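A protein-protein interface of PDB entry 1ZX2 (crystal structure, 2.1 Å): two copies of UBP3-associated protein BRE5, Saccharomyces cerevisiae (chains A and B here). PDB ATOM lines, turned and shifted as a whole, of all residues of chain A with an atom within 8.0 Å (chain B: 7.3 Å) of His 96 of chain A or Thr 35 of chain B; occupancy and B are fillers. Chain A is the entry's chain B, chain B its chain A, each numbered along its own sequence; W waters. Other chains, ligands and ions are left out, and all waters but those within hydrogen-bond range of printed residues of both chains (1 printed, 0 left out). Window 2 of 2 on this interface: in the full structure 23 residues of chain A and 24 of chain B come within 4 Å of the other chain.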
ATOM      1  N   GLN A  90      10.592  28.059   3.743  1.00  0.00           N
ATOM      2  CA  GLN A  90       9.277  27.512   3.450  1.00  0.00           C
ATOM      3  C   GLN A  90       9.353  26.031   3.460  1.00  0.00           C
ATOM      4  O   GLN A  90      10.348  25.474   3.010  1.00  0.00           O
ATOM      5  CB  GLN A  90       8.845  27.916   1.988  1.00  0.00           C
ATOM      6  CG  GLN A  90       8.593  29.397   1.705  1.00  0.00           C
ATOM      7  CD  GLN A  90       8.284  29.635   0.196  1.00  0.00           C
ATOM      8  OE1 GLN A  90       8.485  28.740  -0.609  1.00  0.00           O
ATOM      9  NE2 GLN A  90       7.858  30.847  -0.164  1.00  0.00           N
ATOM     10  N   TYR A  91       8.310  25.394   3.925  1.00  0.00           N
ATOM     11  CA  TYR A  91       8.107  24.018   3.732  1.00  0.00           C
ATOM     12  C   TYR A  91       7.954  23.678   2.213  1.00  0.00           C
ATOM     13  O   TYR A  91       7.473  24.483   1.394  1.00  0.00           O
ATOM     14  CB  TYR A  91       6.904  23.529   4.577  1.00  0.00           C
ATOM     15  CG  TYR A  91       7.237  23.350   6.052  1.00  0.00           C
ATOM     16  CD1 TYR A  91       6.567  24.093   7.052  1.00  0.00           C
ATOM     17  CD2 TYR A  91       8.210  22.404   6.460  1.00  0.00           C
ATOM     18  CE1 TYR A  91       6.902  23.899   8.428  1.00  0.00           C
ATOM     19  CE2 TYR A  91       8.538  22.222   7.844  1.00  0.00           C
ATOM     20  CZ  TYR A  91       7.874  22.977   8.781  1.00  0.00           C
ATOM     21  OH  TYR A  91       8.256  22.770  10.062  1.00  0.00           O
ATOM     22  N   THR A  92       8.403  22.480   1.840  1.00  0.00           N
ATOM     23  CA  THR A  92       8.357  22.021   0.471  1.00  0.00           C
ATOM     24  C   THR A  92       8.347  20.487   0.391  1.00  0.00           C
ATOM     25  O   THR A  92       8.497  19.773   1.409  1.00  0.00           O
ATOM     26  CB  THR A  92       9.539  22.634  -0.259  1.00  0.00           C
ATOM     27  OG1 THR A  92       9.408  22.433  -1.685  1.00  0.00           O
ATOM     28  CG2 THR A  92      10.915  21.980   0.187  1.00  0.00           C
ATOM     29  N   GLY A  93       8.251  19.971  -0.840  1.00  0.00           N
ATOM     30  CA  GLY A  93       8.517  18.578  -1.090  1.00  0.00           C
ATOM     31  C   GLY A  93       7.455  17.658  -0.527  1.00  0.00           C
ATOM     32  O   GLY A  93       6.346  18.056  -0.244  1.00  0.00           O
ATOM     33  N   HIS A  94       7.860  16.432  -0.277  1.00  0.00           N
ATOM     34  CA  HIS A  94       6.948  15.306   0.016  1.00  0.00           C
ATOM     35  C   HIS A  94       6.280  15.585   1.316  1.00  0.00           C
ATOM     36  O   HIS A  94       6.984  15.793   2.328  1.00  0.00           O
ATOM     37  CB  HIS A  94       7.737  13.977   0.090  1.00  0.00           C
ATOM     38  CG  HIS A  94       6.858  12.784   0.259  1.00  0.00           C
ATOM     39  ND1 HIS A  94       6.680  12.165   1.478  1.00  0.00           N
ATOM     40  CD2 HIS A  94       6.039  12.159  -0.614  1.00  0.00           C
ATOM     41  CE1 HIS A  94       5.808  11.185   1.338  1.00  0.00           C
ATOM     42  NE2 HIS A  94       5.412  11.157   0.076  1.00  0.00           N
ATOM     43  N   LEU A  95       4.933  15.676   1.287  1.00  0.00           N
ATOM     44  CA  LEU A  95       4.110  15.955   2.480  1.00  0.00           C
ATOM     45  C   LEU A  95       4.495  17.286   3.178  1.00  0.00           C
ATOM     46  O   LEU A  95       4.207  17.492   4.361  1.00  0.00           O
ATOM     47  CB  LEU A  95       4.167  14.771   3.485  1.00  0.00           C
ATOM     48  CG  LEU A  95       3.646  13.404   3.003  1.00  0.00           C
ATOM     49  CD1 LEU A  95       3.749  12.318   4.059  1.00  0.00           C
ATOM     50  CD2 LEU A  95       2.171  13.492   2.460  1.00  0.00           C
ATOM     51  N   HIS A  96       5.086  18.208   2.422  1.00  0.00           N
ATOM     52  CA  HIS A  96       5.496  19.491   2.977  1.00  0.00           C
ATOM     53  C   HIS A  96       6.429  19.258   4.175  1.00  0.00           C
ATOM     54  O   HIS A  96       6.410  20.016   5.040  1.00  0.00           O
ATOM     55  CB  HIS A  96       4.293  20.463   3.335  1.00  0.00           C
ATOM     56  CG  HIS A  96       3.401  20.742   2.180  1.00  0.00           C
ATOM     57  ND1 HIS A  96       3.839  21.395   1.044  1.00  0.00           N
ATOM     58  CD2 HIS A  96       2.111  20.358   1.927  1.00  0.00           C
ATOM     59  CE1 HIS A  96       2.854  21.417   0.150  1.00  0.00           C
ATOM     60  NE2 HIS A  96       1.793  20.807   0.665  1.00  0.00           N
ATOM     61  N   LYS A  97       7.252  18.212   4.176  1.00  0.00           N
ATOM     62  CA  LYS A  97       8.115  17.940   5.294  1.00  0.00           C
ATOM     63  C   LYS A  97       9.608  18.372   5.066  1.00  0.00           C
ATOM     64  O   LYS A  97      10.388  18.459   6.007  1.00  0.00           O
ATOM     65  CB  LYS A  97       7.999  16.458   5.654  1.00  0.00           C
ATOM     66  CG  LYS A  97       6.685  16.130   6.454  1.00  0.00           C
ATOM     67  CD  LYS A  97       6.527  14.581   6.566  1.00  0.00           C
ATOM     68  CE  LYS A  97       5.260  14.181   7.436  1.00  0.00           C
ATOM     69  NZ  LYS A  97       5.233  12.666   7.661  1.00  0.00           N
ATOM     70  N   SER A  98       9.973  18.696   3.830  1.00  0.00           N
ATOM     71  CA  SER A  98      11.257  19.289   3.545  1.00  0.00           C
ATOM     72  C   SER A  98      11.240  20.787   3.735  1.00  0.00           C
ATOM     73  O   SER A  98      10.178  21.421   3.871  1.00  0.00           O
ATOM     74  CB  SER A  98      11.755  18.885   2.152  1.00  0.00           C
ATOM     75  OG  SER A  98      11.897  17.471   2.029  1.00  0.00           O
ATOM     76  N   ILE A  99      12.433  21.384   3.762  1.00  0.00           N
ATOM     77  CA  ILE A  99      12.545  22.812   3.974  1.00  0.00           C
ATOM     78  C   ILE A  99      13.449  23.453   2.945  1.00  0.00           C
ATOM     79  O   ILE A  99      14.620  23.040   2.731  1.00  0.00           O
ATOM     80  CB  ILE A  99      13.055  23.104   5.401  1.00  0.00           C
ATOM     81  CG1 ILE A  99      12.156  22.475   6.441  1.00  0.00           C
ATOM     82  CG2 ILE A  99      13.112  24.561   5.680  1.00  0.00           C
ATOM     83  CD1 ILE A  99      12.825  22.497   7.769  1.00  0.00           C
ATOM     84  N   PRO A 125      14.054  15.561   5.852  1.00  0.00           N
ATOM     85  CA  PRO A 125      14.153  14.881   7.135  1.00  0.00           C
ATOM     86  C   PRO A 125      14.795  13.507   6.975  1.00  0.00           C
ATOM     87  O   PRO A 125      14.754  12.929   5.894  1.00  0.00           O
ATOM     88  CB  PRO A 125      12.682  14.791   7.631  1.00  0.00           C
ATOM     89  CG  PRO A 125      11.823  15.170   6.554  1.00  0.00           C
ATOM     90  CD  PRO A 125      12.667  15.785   5.467  1.00  0.00           C
ATOM     91  N   PHE A 132      17.870  16.601   9.871  1.00  0.00           N
ATOM     92  CA  PHE A 132      17.674  16.975   8.503  1.00  0.00           C
ATOM     93  C   PHE A 132      19.031  16.815   7.839  1.00  0.00           C
ATOM     94  O   PHE A 132      20.031  17.069   8.503  1.00  0.00           O
ATOM     95  CB  PHE A 132      17.169  18.422   8.462  1.00  0.00           C
ATOM     96  CG  PHE A 132      15.699  18.557   8.840  1.00  0.00           C
ATOM     97  CD1 PHE A 132      15.308  18.701  10.175  1.00  0.00           C
ATOM     98  CD2 PHE A 132      14.729  18.514   7.865  1.00  0.00           C
ATOM     99  CE1 PHE A 132      13.936  18.772  10.510  1.00  0.00           C
ATOM    100  CE2 PHE A 132      13.364  18.632   8.204  1.00  0.00           C
ATOM    101  CZ  PHE A 132      12.980  18.737   9.493  1.00  0.00           C
ATOM    102  N   TYR B  32       1.282  28.257 -10.572  1.00  0.00           N
ATOM    103  CA  TYR B  32       1.507  27.750  -9.247  1.00  0.00           C
ATOM    104  C   TYR B  32       0.666  26.554  -8.941  1.00  0.00           C
ATOM    105  O   TYR B  32      -0.439  26.480  -9.405  1.00  0.00           O
ATOM    106  CB  TYR B  32       1.185  28.854  -8.214  1.00  0.00           C
ATOM    107  CG  TYR B  32       2.151  29.971  -8.252  1.00  0.00           C
ATOM    108  CD1 TYR B  32       3.208  30.055  -7.348  1.00  0.00           C
ATOM    109  CD2 TYR B  32       2.069  30.919  -9.245  1.00  0.00           C
ATOM    110  CE1 TYR B  32       4.086  31.056  -7.402  1.00  0.00           C
ATOM    111  CE2 TYR B  32       2.967  31.921  -9.307  1.00  0.00           C
ATOM    112  CZ  TYR B  32       3.950  32.024  -8.339  1.00  0.00           C
ATOM    113  OH  TYR B  32       4.856  33.067  -8.428  1.00  0.00           O
ATOM    114  N   ALA B  33       1.179  25.597  -8.169  1.00  0.00           N
ATOM    115  CA  ALA B  33       0.313  24.557  -7.596  1.00  0.00           C
ATOM    116  C   ALA B  33      -0.749  25.135  -6.666  1.00  0.00           C
ATOM    117  O   ALA B  33      -0.589  26.228  -6.097  1.00  0.00           O
ATOM    118  CB  ALA B  33       1.177  23.497  -6.871  1.00  0.00           C
ATOM    119  N   SER B  34      -1.805  24.384  -6.427  1.00  0.00           N
ATOM    120  CA  SER B  34      -2.900  24.941  -5.663  1.00  0.00           C
ATOM    121  C   SER B  34      -2.468  25.340  -4.262  1.00  0.00           C
ATOM    122  O   SER B  34      -3.067  26.229  -3.690  1.00  0.00           O
ATOM    123  CB  SER B  34      -4.087  23.954  -5.544  1.00  0.00           C
ATOM    124  OG  SER B  34      -3.508  22.721  -5.144  1.00  0.00           O
ATOM    125  N   THR B  35      -1.477  24.662  -3.682  1.00  0.00           N
ATOM    126  CA  THR B  35      -1.081  24.936  -2.316  1.00  0.00           C
ATOM    127  C   THR B  35       0.330  25.579  -2.253  1.00  0.00           C
ATOM    128  O   THR B  35       0.957  25.509  -1.224  1.00  0.00           O
ATOM    129  CB  THR B  35      -1.079  23.626  -1.398  1.00  0.00           C
ATOM    130  OG1 THR B  35      -0.095  22.679  -1.912  1.00  0.00           O
ATOM    131  CG2 THR B  35      -2.478  22.883  -1.424  1.00  0.00           C
ATOM    132  N   ALA B  36       0.757  26.239  -3.334  1.00  0.00           N
ATOM    133  CA  ALA B  36       2.060  26.876  -3.391  1.00  0.00           C
ATOM    134  C   ALA B  36       2.250  27.969  -2.319  1.00  0.00           C
ATOM    135  O   ALA B  36       1.286  28.590  -1.858  1.00  0.00           O
ATOM    136  CB  ALA B  36       2.257  27.500  -4.705  1.00  0.00           C
ATOM    137  N   GLU B  37       3.509  28.206  -1.948  1.00  0.00           N
ATOM    138  CA  GLU B  37       3.833  29.301  -1.052  1.00  0.00           C
ATOM    139  C   GLU B  37       4.677  30.291  -1.731  1.00  0.00           C
ATOM    140  O   GLU B  37       5.620  29.934  -2.441  1.00  0.00           O
ATOM    141  CB  GLU B  37       4.684  28.804   0.062  1.00  0.00           C
ATOM    142  CG  GLU B  37       3.938  27.926   0.958  1.00  0.00           C
ATOM    143  CD  GLU B  37       4.866  27.420   2.004  1.00  0.00           C
ATOM    144  OE1 GLU B  37       5.076  26.121   1.915  1.00  0.00           O
ATOM    145  OE2 GLU B  37       5.370  28.356   2.793  1.00  0.00           O
ATOM    146  N   LEU B  38       4.353  31.550  -1.496  1.00  0.00           N
ATOM    147  CA  LEU B  38       5.048  32.642  -2.113  1.00  0.00           C
ATOM    148  C   LEU B  38       5.528  33.557  -1.025  1.00  0.00           C
ATOM    149  O   LEU B  38       4.757  33.944  -0.123  1.00  0.00           O
ATOM    150  CB  LEU B  38       4.073  33.410  -3.005  1.00  0.00           C
ATOM    151  CG  LEU B  38       4.541  34.690  -3.636  1.00  0.00           C
ATOM    152  CD1 LEU B  38       5.219  34.379  -4.867  1.00  0.00           C
ATOM    153  CD2 LEU B  38       3.399  35.522  -3.963  1.00  0.00           C
ATOM    154  N   VAL B  60       2.257  34.498   1.265  1.00  0.00           N
ATOM    155  CA  VAL B  60       0.935  33.967   0.990  1.00  0.00           C
ATOM    156  C   VAL B  60       0.964  32.533   0.569  1.00  0.00           C
ATOM    157  O   VAL B  60       1.962  32.034   0.024  1.00  0.00           O
ATOM    158  CB  VAL B  60       0.122  34.807  -0.020  1.00  0.00           C
ATOM    159  CG1 VAL B  60       0.186  36.301   0.330  1.00  0.00           C
ATOM    160  CG2 VAL B  60       0.537  34.644  -1.318  1.00  0.00           C
ATOM    161  N   THR B  61      -0.131  31.865   0.878  1.00  0.00           N
ATOM    162  CA  THR B  61      -0.288  30.446   0.591  1.00  0.00           C
ATOM    163  C   THR B  61      -1.535  30.216  -0.219  1.00  0.00           C
ATOM    164  O   THR B  61      -2.553  30.749   0.115  1.00  0.00           O
ATOM    165  CB  THR B  61      -0.322  29.612   1.924  1.00  0.00           C
ATOM    166  OG1 THR B  61       0.987  29.628   2.524  1.00  0.00           O
ATOM    167  CG2 THR B  61      -0.434  28.169   1.614  1.00  0.00           C
ATOM    168  N   GLY B  62      -1.420  29.417  -1.284  1.00  0.00           N
ATOM    169  CA  GLY B  62      -2.552  28.863  -2.019  1.00  0.00           C
ATOM    170  C   GLY B  62      -2.757  29.635  -3.310  1.00  0.00           C
ATOM    171  O   GLY B  62      -2.501  30.849  -3.344  1.00  0.00           O
ATOM    172  N   ARG B  63      -3.212  29.002  -4.400  1.00  0.00           N
ATOM    173  CA  ARG B  63      -3.255  29.723  -5.658  1.00  0.00           C
ATOM    174  C   ARG B  63      -4.185  30.926  -5.607  1.00  0.00           C
ATOM    175  O   ARG B  63      -3.870  31.922  -6.226  1.00  0.00           O
ATOM    176  CB  ARG B  63      -3.727  28.842  -6.810  1.00  0.00           C
ATOM    177  CG  ARG B  63      -3.570  29.429  -8.224  1.00  0.00           C
ATOM    178  CD  ARG B  63      -2.911  28.322  -9.239  1.00  0.00           C
ATOM    179  NE  ARG B  63      -3.900  27.412  -9.306  1.00  0.00           N
ATOM    180  CZ  ARG B  63      -3.983  26.157  -9.246  1.00  0.00           C
ATOM    181  NH1 ARG B  63      -3.041  25.243  -9.419  1.00  0.00           N
ATOM    182  NH2 ARG B  63      -5.267  25.799  -9.242  1.00  0.00           N
ATOM    183  N   ILE B  66      -2.413  33.784  -3.981  1.00  0.00           N
ATOM    184  CA  ILE B  66      -1.369  34.240  -4.874  1.00  0.00           C
ATOM    185  C   ILE B  66      -1.918  35.087  -6.000  1.00  0.00           C
ATOM    186  O   ILE B  66      -1.317  36.076  -6.400  1.00  0.00           O
ATOM    187  CB  ILE B  66      -0.578  33.036  -5.395  1.00  0.00           C
ATOM    188  CG1 ILE B  66       0.274  32.423  -4.270  1.00  0.00           C
ATOM    189  CG2 ILE B  66       0.296  33.434  -6.566  1.00  0.00           C
ATOM    190  CD1 ILE B  66       0.727  30.967  -4.497  1.00  0.00           C
ATOM    191  N   ILE B 134       4.894  25.631  -9.863  1.00  0.00           N
ATOM    192  CA  ILE B 134       5.649  26.248  -8.786  1.00  0.00           C
ATOM    193  C   ILE B 134       4.987  25.855  -7.496  1.00  0.00           C
ATOM    194  O   ILE B 134       3.800  26.135  -7.263  1.00  0.00           O
ATOM    195  CB  ILE B 134       5.638  27.716  -8.889  1.00  0.00           C
ATOM    196  CG1 ILE B 134       6.129  28.163 -10.269  1.00  0.00           C
ATOM    197  CG2 ILE B 134       6.506  28.333  -7.827  1.00  0.00           C
ATOM    198  CD1 ILE B 134       5.931  29.663 -10.590  1.00  0.00           C
ATOM    199  N   THR B 135       5.755  25.213  -6.613  1.00  0.00           N
ATOM    200  CA  THR B 135       5.310  24.972  -5.224  1.00  0.00           C
ATOM    201  C   THR B 135       5.873  25.986  -4.230  1.00  0.00           C
ATOM    202  O   THR B 135       5.325  26.219  -3.123  1.00  0.00           O
ATOM    203  CB  THR B 135       5.624  23.543  -4.725  1.00  0.00           C
ATOM    204  OG1 THR B 135       7.044  23.326  -4.783  1.00  0.00           O
ATOM    205  CG2 THR B 135       4.935  22.515  -5.606  1.00  0.00           C
ATOM    206  N   ASN B 136       6.947  26.645  -4.635  1.00  0.00           N
ATOM    207  CA  ASN B 136       7.651  27.567  -3.788  1.00  0.00           C
ATOM    208  C   ASN B 136       8.240  28.629  -4.601  1.00  0.00           C
ATOM    209  O   ASN B 136       8.838  28.398  -5.611  1.00  0.00           O
ATOM    210  CB  ASN B 136       8.832  26.820  -3.066  1.00  0.00           C
ATOM    211  CG  ASN B 136       8.362  25.781  -2.134  1.00  0.00           C
ATOM    212  OD1 ASN B 136       8.078  26.036  -0.905  1.00  0.00           O
ATOM    213  ND2 ASN B 136       8.201  24.575  -2.662  1.00  0.00           N
HETATM  214  O   HOH W   1       7.427  20.653  -3.711  1.00  0.00           O
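The side-chain amide nitrogen of Gln 90 of chain A sits at hydrogen-bond distance from the backbone carbonyl oxygen of Glu 37 of chain B. O of Tyr 91 of chain A sits close to OE1 of Glu 37 of chain B (2.9 Å). The side-chain amide nitrogen (ND2) of Asn 136 of chain B sits at hydrogen-bond distance from the side-chain hydroxyl (OG1) of Thr 92 of chain A (2.6 Å). The side-chain amide oxygen (OD1) of Asn 136 of chain B sits close to the backbone carbonyl oxygen (O) of Tyr 91 of chain A (2.8 Å). OD1 of Asn 136 of chain B sits close to OE1 of Gln 90 of chain A (2.8 Å).
The side-chain hydroxyl (OG1) of Thr 135 of chain B sits at hydrogen-bond distance from the side-chain amide nitrogen (ND2) of Asn 136 of chain B (2.7 Å). O of Thr 92 of chain A sits at hydrogen-bond distance from N of Lys 97 of chain A. The backbone NH of Glu 37 of chain B lies within hydrogen-bond range of the backbone carbonyl oxygen of Thr 135 of chain B, at 2.9 Å. N of Leu 38 of chain B sits at hydrogen-bond distance from O of Val 60 of chain B (2.9 Å). The backbone NH (N) of Thr 92 of chain A is in hydrogen-bond range of the backbone carbonyl oxygen (O) of Ser 98 of chain A (2.9 Å).
Gln 90 of chain A touches Leu 38 of chain B (NE2 to C, 3.7 Å). Thr 135 of chain B touches Thr 92 of chain A. His 96 of chain A touches Thr 35 of chain B.
Printed residues of chain B within 4 Å of Gln 90 of chain A: Glu 37 (3.3 Å), Leu 38 (3.7 Å) and Asn 136 (2.8 Å). No residue of chain A comes within 4 Å of Ser 34 of chain B. Of chain A, only His 96 comes within 4 Å of Thr 35 of chain B. No residue of chain A comes within 4 Å of Ala 36 of chain B. Of the printed residues of chain A, Glu 37 of chain B touches Gln 90 and Tyr 91. Of the printed residues of chain A, Leu 38 of chain B touches Gln 90 (3.7 Å). The nearest residue of chain B that does not touch His 96 of chain A is Glu 37 of chain B (5.0 Å).
Along chain A the printed residues that touch a printed residue of chain B span positions 90 to 96. Among the printed residues, 8 pairs touch across the chains. Among the printed residues, no Asp or Glu carboxylate lies within 4 Å of a Lys or Arg side-chain nitrogen of the other chain.
No position is printed for both chains.
Water W1 lies within hydrogen-bond range of OG1 of Thr 135 of chain B (2.9 Å), N of Gly 93 of chain A (3.1 Å) and OG1 of Thr 92 of chain A (3.3 Å).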
